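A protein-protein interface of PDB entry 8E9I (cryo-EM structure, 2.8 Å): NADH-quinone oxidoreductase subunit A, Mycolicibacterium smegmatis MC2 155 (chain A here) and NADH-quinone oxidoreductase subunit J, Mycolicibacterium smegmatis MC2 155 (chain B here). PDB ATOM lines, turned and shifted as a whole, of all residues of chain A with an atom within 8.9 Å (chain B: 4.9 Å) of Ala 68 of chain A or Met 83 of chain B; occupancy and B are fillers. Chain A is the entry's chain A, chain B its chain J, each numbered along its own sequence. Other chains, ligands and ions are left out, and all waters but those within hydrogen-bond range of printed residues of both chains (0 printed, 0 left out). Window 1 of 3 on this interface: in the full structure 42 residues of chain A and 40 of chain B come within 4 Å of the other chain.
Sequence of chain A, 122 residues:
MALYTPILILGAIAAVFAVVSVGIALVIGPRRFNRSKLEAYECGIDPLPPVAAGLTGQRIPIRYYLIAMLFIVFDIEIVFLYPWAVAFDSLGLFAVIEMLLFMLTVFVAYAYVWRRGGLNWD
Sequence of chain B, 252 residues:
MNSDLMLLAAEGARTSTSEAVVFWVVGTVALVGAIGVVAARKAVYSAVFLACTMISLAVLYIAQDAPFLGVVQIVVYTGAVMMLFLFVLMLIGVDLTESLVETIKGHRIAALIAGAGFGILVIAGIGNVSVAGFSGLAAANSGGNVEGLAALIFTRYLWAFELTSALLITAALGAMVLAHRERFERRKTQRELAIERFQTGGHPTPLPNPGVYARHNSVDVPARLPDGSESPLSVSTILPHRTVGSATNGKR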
ATOM      1  N   ILE A  62      -5.337  -8.036   6.688  1.00  0.00           N
ATOM      2  CA  ILE A  62      -6.325  -8.112   7.753  1.00  0.00           C
ATOM      3  C   ILE A  62      -5.666  -8.787   8.943  1.00  0.00           C
ATOM      4  O   ILE A  62      -4.930  -9.766   8.782  1.00  0.00           O
ATOM      5  CB  ILE A  62      -7.602  -8.853   7.318  1.00  0.00           C
ATOM      6  CG1 ILE A  62      -7.381 -10.364   7.165  1.00  0.00           C
ATOM      7  CG2 ILE A  62      -8.119  -8.261   6.017  1.00  0.00           C
ATOM      8  CD1 ILE A  62      -8.665 -11.154   7.151  1.00  0.00           C
ATOM      9  N   ARG A  63      -5.916  -8.250  10.133  1.00  0.00           N
ATOM     10  CA  ARG A  63      -5.283  -8.777  11.329  1.00  0.00           C
ATOM     11  C   ARG A  63      -6.002  -9.997  11.877  1.00  0.00           C
ATOM     12  O   ARG A  63      -5.529 -10.600  12.845  1.00  0.00           O
ATOM     13  CB  ARG A  63      -5.208  -7.685  12.392  1.00  0.00           C
ATOM     14  CG  ARG A  63      -4.704  -6.371  11.839  1.00  0.00           C
ATOM     15  CD  ARG A  63      -4.677  -5.283  12.877  1.00  0.00           C
ATOM     16  NE  ARG A  63      -3.839  -5.641  14.016  1.00  0.00           N
ATOM     17  CZ  ARG A  63      -4.257  -5.745  15.272  1.00  0.00           C
ATOM     18  NH1 ARG A  63      -5.503  -5.458  15.619  1.00  0.00           N
ATOM     19  NH2 ARG A  63      -3.400  -6.139  16.208  1.00  0.00           N
ATOM     20  N   TYR A  64      -7.125 -10.380  11.281  1.00  0.00           N
ATOM     21  CA  TYR A  64      -7.909 -11.505  11.757  1.00  0.00           C
ATOM     22  C   TYR A  64      -7.956 -12.650  10.759  1.00  0.00           C
ATOM     23  O   TYR A  64      -8.911 -13.432  10.775  1.00  0.00           O
ATOM     24  CB  TYR A  64      -9.321 -11.041  12.094  1.00  0.00           C
ATOM     25  CG  TYR A  64     -10.040 -10.368  10.957  1.00  0.00           C
ATOM     26  CD1 TYR A  64      -9.880  -9.013  10.716  1.00  0.00           C
ATOM     27  CD2 TYR A  64     -10.898 -11.081  10.140  1.00  0.00           C
ATOM     28  CE1 TYR A  64     -10.539  -8.391   9.682  1.00  0.00           C
ATOM     29  CE2 TYR A  64     -11.564 -10.470   9.106  1.00  0.00           C
ATOM     30  CZ  TYR A  64     -11.382  -9.127   8.881  1.00  0.00           C
ATOM     31  OH  TYR A  64     -12.050  -8.525   7.845  1.00  0.00           O
ATOM     32  N   TYR A  65      -6.946 -12.772   9.897  1.00  0.00           N
ATOM     33  CA  TYR A  65      -6.917 -13.892   8.966  1.00  0.00           C
ATOM     34  C   TYR A  65      -7.110 -15.207   9.698  1.00  0.00           C
ATOM     35  O   TYR A  65      -7.806 -16.104   9.211  1.00  0.00           O
ATOM     36  CB  TYR A  65      -5.602 -13.899   8.182  1.00  0.00           C
ATOM     37  CG  TYR A  65      -4.369 -13.701   9.031  1.00  0.00           C
ATOM     38  CD1 TYR A  65      -3.912 -14.692   9.882  1.00  0.00           C
ATOM     39  CD2 TYR A  65      -3.669 -12.506   8.991  1.00  0.00           C
ATOM     40  CE1 TYR A  65      -2.792 -14.502  10.662  1.00  0.00           C
ATOM     41  CE2 TYR A  65      -2.551 -12.311   9.765  1.00  0.00           C
ATOM     42  CZ  TYR A  65      -2.120 -13.309  10.602  1.00  0.00           C
ATOM     43  OH  TYR A  65      -1.000 -13.114  11.372  1.00  0.00           O
ATOM     44  N   LEU A  66      -6.521 -15.333  10.882  1.00  0.00           N
ATOM     45  CA  LEU A  66      -6.644 -16.576  11.625  1.00  0.00           C
ATOM     46  C   LEU A  66      -8.088 -16.820  12.032  1.00  0.00           C
ATOM     47  O   LEU A  66      -8.603 -17.935  11.897  1.00  0.00           O
ATOM     48  CB  LEU A  66      -5.735 -16.532  12.845  1.00  0.00           C
ATOM     49  CG  LEU A  66      -5.762 -17.741  13.767  1.00  0.00           C
ATOM     50  CD1 LEU A  66      -5.685 -19.042  13.003  1.00  0.00           C
ATOM     51  CD2 LEU A  66      -4.606 -17.613  14.711  1.00  0.00           C
ATOM     52  N   ILE A  67      -8.767 -15.781  12.513  1.00  0.00           N
ATOM     53  CA  ILE A  67     -10.158 -15.949  12.908  1.00  0.00           C
ATOM     54  C   ILE A  67     -11.031 -16.173  11.686  1.00  0.00           C
ATOM     55  O   ILE A  67     -12.038 -16.874  11.756  1.00  0.00           O
ATOM     56  CB  ILE A  67     -10.632 -14.750  13.746  1.00  0.00           C
ATOM     57  CG1 ILE A  67      -9.721 -14.604  14.967  1.00  0.00           C
ATOM     58  CG2 ILE A  67     -12.080 -14.949  14.161  1.00  0.00           C
ATOM     59  CD1 ILE A  67     -10.132 -13.556  15.964  1.00  0.00           C
ATOM     60  N   ALA A  68     -10.662 -15.595  10.542  1.00  0.00           N
ATOM     61  CA  ALA A  68     -11.410 -15.863   9.317  1.00  0.00           C
ATOM     62  C   ALA A  68     -11.306 -17.331   8.918  1.00  0.00           C
ATOM     63  O   ALA A  68     -12.315 -17.978   8.593  1.00  0.00           O
ATOM     64  CB  ALA A  68     -10.899 -14.967   8.191  1.00  0.00           C
ATOM     65  N   MET A  69     -10.089 -17.870   8.937  1.00  0.00           N
ATOM     66  CA  MET A  69      -9.887 -19.284   8.657  1.00  0.00           C
ATOM     67  C   MET A  69     -10.678 -20.143   9.631  1.00  0.00           C
ATOM     68  O   MET A  69     -11.368 -21.088   9.233  1.00  0.00           O
ATOM     69  CB  MET A  69      -8.397 -19.608   8.743  1.00  0.00           C
ATOM     70  CG  MET A  69      -7.556 -18.833   7.746  1.00  0.00           C
ATOM     71  SD  MET A  69      -5.782 -19.059   7.942  1.00  0.00           S
ATOM     72  CE  MET A  69      -5.651 -20.833   7.892  1.00  0.00           C
ATOM     73  N   LEU A  70     -10.592 -19.825  10.921  1.00  0.00           N
ATOM     74  CA  LEU A  70     -11.330 -20.596  11.910  1.00  0.00           C
ATOM     75  C   LEU A  70     -12.829 -20.468  11.692  1.00  0.00           C
ATOM     76  O   LEU A  70     -13.580 -21.413  11.942  1.00  0.00           O
ATOM     77  CB  LEU A  70     -10.947 -20.142  13.314  1.00  0.00           C
ATOM     78  CG  LEU A  70      -9.474 -20.358  13.642  1.00  0.00           C
ATOM     79  CD1 LEU A  70      -9.009 -19.330  14.654  1.00  0.00           C
ATOM     80  CD2 LEU A  70      -9.251 -21.771  14.152  1.00  0.00           C
ATOM     81  N   PHE A  71     -13.280 -19.301  11.234  1.00  0.00           N
ATOM     82  CA  PHE A  71     -14.694 -19.090  10.965  1.00  0.00           C
ATOM     83  C   PHE A  71     -15.170 -20.017   9.865  1.00  0.00           C
ATOM     84  O   PHE A  71     -16.250 -20.599   9.952  1.00  0.00           O
ATOM     85  CB  PHE A  71     -14.938 -17.630  10.581  1.00  0.00           C
ATOM     86  CG  PHE A  71     -16.170 -17.419   9.749  1.00  0.00           C
ATOM     87  CD1 PHE A  71     -17.411 -17.290  10.345  1.00  0.00           C
ATOM     88  CD2 PHE A  71     -16.085 -17.347   8.374  1.00  0.00           C
ATOM     89  CE1 PHE A  71     -18.539 -17.099   9.584  1.00  0.00           C
ATOM     90  CE2 PHE A  71     -17.211 -17.155   7.610  1.00  0.00           C
ATOM     91  CZ  PHE A  71     -18.439 -17.032   8.214  1.00  0.00           C
ATOM     92  N   ILE A  72     -14.370 -20.166   8.811  1.00  0.00           N
ATOM     93  CA  ILE A  72     -14.747 -21.095   7.747  1.00  0.00           C
ATOM     94  C   ILE A  72     -15.138 -22.443   8.343  1.00  0.00           C
ATOM     95  O   ILE A  72     -16.286 -22.906   8.222  1.00  0.00           O
ATOM     96  CB  ILE A  72     -13.595 -21.252   6.740  1.00  0.00           C
ATOM     97  CG1 ILE A  72     -13.317 -19.926   6.037  1.00  0.00           C
ATOM     98  CG2 ILE A  72     -13.923 -22.340   5.736  1.00  0.00           C
ATOM     99  CD1 ILE A  72     -12.012 -19.900   5.267  1.00  0.00           C
ATOM    100  N   VAL A  73     -14.185 -23.071   9.030  1.00  0.00           N
ATOM    101  CA  VAL A  73     -14.377 -24.422   9.539  1.00  0.00           C
ATOM    102  C   VAL A  73     -15.481 -24.462  10.587  1.00  0.00           C
ATOM    103  O   VAL A  73     -16.316 -25.368  10.582  1.00  0.00           O
ATOM    104  CB  VAL A  73     -13.052 -24.982  10.095  1.00  0.00           C
ATOM    105  CG1 VAL A  73     -12.078 -25.246   8.961  1.00  0.00           C
ATOM    106  CG2 VAL A  73     -12.440 -24.042  11.123  1.00  0.00           C
ATOM    107  N   PHE A  74     -15.510 -23.500  11.507  1.00  0.00           N
ATOM    108  CA  PHE A  74     -16.507 -23.559  12.567  1.00  0.00           C
ATOM    109  C   PHE A  74     -17.909 -23.373  12.012  1.00  0.00           C
ATOM    110  O   PHE A  74     -18.836 -24.094  12.397  1.00  0.00           O
ATOM    111  CB  PHE A  74     -16.202 -22.513  13.634  1.00  0.00           C
ATOM    112  CG  PHE A  74     -15.109 -22.920  14.573  1.00  0.00           C
ATOM    113  CD1 PHE A  74     -15.234 -24.059  15.344  1.00  0.00           C
ATOM    114  CD2 PHE A  74     -13.956 -22.168  14.683  1.00  0.00           C
ATOM    115  CE1 PHE A  74     -14.223 -24.445  16.206  1.00  0.00           C
ATOM    116  CE2 PHE A  74     -12.944 -22.545  15.542  1.00  0.00           C
ATOM    117  CZ  PHE A  74     -13.079 -23.686  16.304  1.00  0.00           C
ATOM    118  N   ASP A  75     -18.092 -22.415  11.105  1.00  0.00           N
ATOM    119  CA  ASP A  75     -19.404 -22.204  10.513  1.00  0.00           C
ATOM    120  C   ASP A  75     -19.884 -23.466   9.816  1.00  0.00           C
ATOM    121  O   ASP A  75     -21.030 -23.885   9.997  1.00  0.00           O
ATOM    122  CB  ASP A  75     -19.359 -21.034   9.533  1.00  0.00           C
ATOM    123  N   GLY A 118      -4.914 -17.606  19.430  1.00  0.00           N
ATOM    124  CA  GLY A 118      -5.383 -17.519  18.059  1.00  0.00           C
ATOM    125  C   GLY A 118      -6.415 -16.432  17.857  1.00  0.00           C
ATOM    126  O   GLY A 118      -6.485 -15.831  16.784  1.00  0.00           O
ATOM    127  N   LEU A 119      -7.217 -16.155  18.879  1.00  0.00           N
ATOM    128  CA  LEU A 119      -8.282 -15.171  18.768  1.00  0.00           C
ATOM    129  C   LEU A 119      -7.839 -13.769  19.152  1.00  0.00           C
ATOM    130  O   LEU A 119      -8.668 -12.854  19.146  1.00  0.00           O
ATOM    131  CB  LEU A 119      -9.456 -15.582  19.654  1.00  0.00           C
ATOM    132  CG  LEU A 119      -9.956 -17.009  19.436  1.00  0.00           C
ATOM    133  CD1 LEU A 119     -11.099 -17.328  20.375  1.00  0.00           C
ATOM    134  CD2 LEU A 119     -10.376 -17.201  17.996  1.00  0.00           C
ATOM    135  N   ASP A 122      -6.835  -9.903  16.671  1.00  0.00           N
ATOM    136  CA  ASP A 122      -7.882  -8.931  16.380  1.00  0.00           C
ATOM    137  C   ASP A 122      -9.074  -9.168  17.300  1.00  0.00           C
ATOM    138  O   ASP A 122      -9.154  -8.624  18.402  1.00  0.00           O
ATOM    139  CB  ASP A 122      -8.333  -9.008  14.930  1.00  0.00           C
ATOM    140  CG  ASP A 122      -8.937  -7.711  14.443  1.00  0.00           C
ATOM    141  OD1 ASP A 122      -8.253  -6.672  14.510  1.00  0.00           O
ATOM    142  OD2 ASP A 122     -10.105  -7.731  14.009  1.00  0.00           O
ATOM    143  OXT ASP A 122      -9.990  -9.917  16.964  1.00  0.00           O
ATOM    144  N   GLY B  79     -20.216 -17.478   3.669  1.00  0.00           N
ATOM    145  CA  GLY B  79     -19.095 -17.297   4.572  1.00  0.00           C
ATOM    146  C   GLY B  79     -17.760 -17.579   3.908  1.00  0.00           C
ATOM    147  O   GLY B  79     -16.805 -16.801   4.023  1.00  0.00           O
ATOM    148  N   ALA B  80     -17.697 -18.699   3.191  1.00  0.00           N
ATOM    149  CA  ALA B  80     -16.437 -19.151   2.617  1.00  0.00           C
ATOM    150  C   ALA B  80     -15.939 -18.188   1.552  1.00  0.00           C
ATOM    151  O   ALA B  80     -14.749 -17.868   1.501  1.00  0.00           O
ATOM    152  CB  ALA B  80     -16.602 -20.551   2.031  1.00  0.00           C
ATOM    153  N   VAL B  81     -16.832 -17.731   0.674  1.00  0.00           N
ATOM    154  CA  VAL B  81     -16.412 -16.818  -0.375  1.00  0.00           C
ATOM    155  C   VAL B  81     -16.102 -15.450   0.202  1.00  0.00           C
ATOM    156  O   VAL B  81     -15.232 -14.744  -0.312  1.00  0.00           O
ATOM    157  CB  VAL B  81     -17.466 -16.739  -1.489  1.00  0.00           C
ATOM    158  CG1 VAL B  81     -16.998 -15.785  -2.565  1.00  0.00           C
ATOM    159  CG2 VAL B  81     -17.708 -18.112  -2.080  1.00  0.00           C
ATOM    160  N   MET B  82     -16.773 -15.047   1.280  1.00  0.00           N
ATOM    161  CA  MET B  82     -16.349 -13.824   1.945  1.00  0.00           C
ATOM    162  C   MET B  82     -14.912 -13.943   2.429  1.00  0.00           C
ATOM    163  O   MET B  82     -14.099 -13.038   2.202  1.00  0.00           O
ATOM    164  CB  MET B  82     -17.281 -13.511   3.111  1.00  0.00           C
ATOM    165  N   MET B  83     -14.572 -15.054   3.081  1.00  0.00           N
ATOM    166  CA  MET B  83     -13.199 -15.214   3.552  1.00  0.00           C
ATOM    167  C   MET B  83     -12.217 -15.324   2.393  1.00  0.00           C
ATOM    168  O   MET B  83     -11.105 -14.796   2.469  1.00  0.00           O
ATOM    169  CB  MET B  83     -13.071 -16.437   4.458  1.00  0.00           C
ATOM    170  CG  MET B  83     -14.055 -16.504   5.611  1.00  0.00           C
ATOM    171  SD  MET B  83     -14.058 -15.086   6.716  1.00  0.00           S
ATOM    172  CE  MET B  83     -15.037 -13.907   5.795  1.00  0.00           C
ATOM    173  N   LEU B  84     -12.591 -16.021   1.323  1.00  0.00           N
ATOM    174  CA  LEU B  84     -11.700 -16.124   0.175  1.00  0.00           C
ATOM    175  C   LEU B  84     -11.494 -14.764  -0.472  1.00  0.00           C
ATOM    176  O   LEU B  84     -10.416 -14.476  -0.995  1.00  0.00           O
ATOM    177  CB  LEU B  84     -12.257 -17.120  -0.836  1.00  0.00           C
ATOM    178  CG  LEU B  84     -12.133 -18.579  -0.405  1.00  0.00           C
ATOM    179  CD1 LEU B  84     -13.023 -19.461  -1.251  1.00  0.00           C
ATOM    180  CD2 LEU B  84     -10.689 -19.039  -0.472  1.00  0.00           C
ATOM    181  N   PHE B  85     -12.517 -13.913  -0.444  1.00  0.00           N
ATOM    182  CA  PHE B  85     -12.365 -12.549  -0.930  1.00  0.00           C
ATOM    183  C   PHE B  85     -11.410 -11.764  -0.045  1.00  0.00           C
ATOM    184  O   PHE B  85     -10.563 -11.009  -0.536  1.00  0.00           O
ATOM    185  CB  PHE B  85     -13.736 -11.879  -0.995  1.00  0.00           C
ATOM    186  CG  PHE B  85     -13.683 -10.384  -1.030  1.00  0.00           C
ATOM    187  CD1 PHE B  85     -13.669  -9.649   0.140  1.00  0.00           C
ATOM    188  CD2 PHE B  85     -13.654  -9.713  -2.235  1.00  0.00           C
ATOM    189  CE1 PHE B  85     -13.625  -8.278   0.105  1.00  0.00           C
ATOM    190  CE2 PHE B  85     -13.606  -8.342  -2.273  1.00  0.00           C
ATOM    191  CZ  PHE B  85     -13.595  -7.623  -1.104  1.00  0.00           C
ATOM    192  N   LEU B  86     -11.533 -11.927   1.270  1.00  0.00           N
ATOM    193  CA  LEU B  86     -10.583 -11.287   2.174  1.00  0.00           C
ATOM    194  C   LEU B  86      -9.162 -11.737   1.873  1.00  0.00           C
ATOM    195  O   LEU B  86      -8.230 -10.927   1.859  1.00  0.00           O
ATOM    196  CB  LEU B  86     -10.930 -11.609   3.623  1.00  0.00           C
ATOM    197  CG  LEU B  86     -12.082 -10.840   4.258  1.00  0.00           C
ATOM    198  CD1 LEU B  86     -12.327 -11.372   5.650  1.00  0.00           C
ATOM    199  CD2 LEU B  86     -11.785  -9.358   4.301  1.00  0.00           C
ATOM    200  N   PHE B  87      -8.978 -13.031   1.638  1.00  0.00           N
ATOM    201  CA  PHE B  87      -7.646 -13.544   1.355  1.00  0.00           C
ATOM    202  C   PHE B  87      -7.161 -13.101  -0.017  1.00  0.00           C
ATOM    203  O   PHE B  87      -5.954 -12.960  -0.228  1.00  0.00           O
ATOM    204  CB  PHE B  87      -7.642 -15.063   1.478  1.00  0.00           C
ATOM    205  CG  PHE B  87      -7.501 -15.541   2.882  1.00  0.00           C
ATOM    206  CD1 PHE B  87      -6.283 -15.489   3.520  1.00  0.00           C
ATOM    207  CD2 PHE B  87      -8.593 -16.013   3.580  1.00  0.00           C
ATOM    208  CE1 PHE B  87      -6.150 -15.917   4.814  1.00  0.00           C
ATOM    209  CE2 PHE B  87      -8.463 -16.442   4.878  1.00  0.00           C
ATOM    210  CZ  PHE B  87      -7.241 -16.394   5.493  1.00  0.00           C
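Ile 62 of chain A touches Leu 86 of chain B.
Tyr 64 of chain A touches Leu 86 of chain B (OH to CD1, 3.6 Å).
Tyr 65 of chain A touches Phe 87 of chain B.
CB of Ala 68 of chain A touches SD of Met 83 of chain B, at 3.5 Å.
Met 69 of chain A touches Phe 87 of chain B (CG to CZ, 3.3 Å).
Gly 79 of chain B touches Phe 71 of chain A.
Met 83 of chain B touches Phe 71 of chain A (SD to CD2, 3.5 Å).
CG1 of Ile 72 of chain A touches CG of Met 83 of chain B, 3.5 Å away.
Of chain A, only Ala 68 (3.5 Å), Phe 71 (3.5 Å) and Ile 72 (3.5 Å) come within 4 Å of Met 83 of chain B.
No residue of chain A comes within 4 Å of Met 82 of chain B.
Of the printed residues of chain A, Gly 79 of chain B touches Phe 71 (3.6 Å).
Of the printed residues of chain B, Met 69 of chain A touches Phe 87.
Of the printed residues of chain A, Phe 87 of chain B touches Tyr 65 and Met 69.
Asp 122 of chain A touches none of the printed residues of chain B.
The nearest printed residue of chain B that does not touch Ile 62 of chain A is Phe 87 of chain B (5.7 Å).
Of the 9 printed residues of chain B, 4 touch a printed residue of chain A.
Hydrophobic or aromatic side chains of chain B within 4 Å of the printed part of chain A: Met 83, Leu 86 and Phe 87.
Along chain B the printed residues that touch a printed residue of chain A span positions 79 to 87.
Among the printed residues, 8 pairs touch across the chains.
Among the printed residues, no Asp or Glu carboxylate lies within 4 Å of a Lys or Arg side-chain nitrogen of the other chain.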
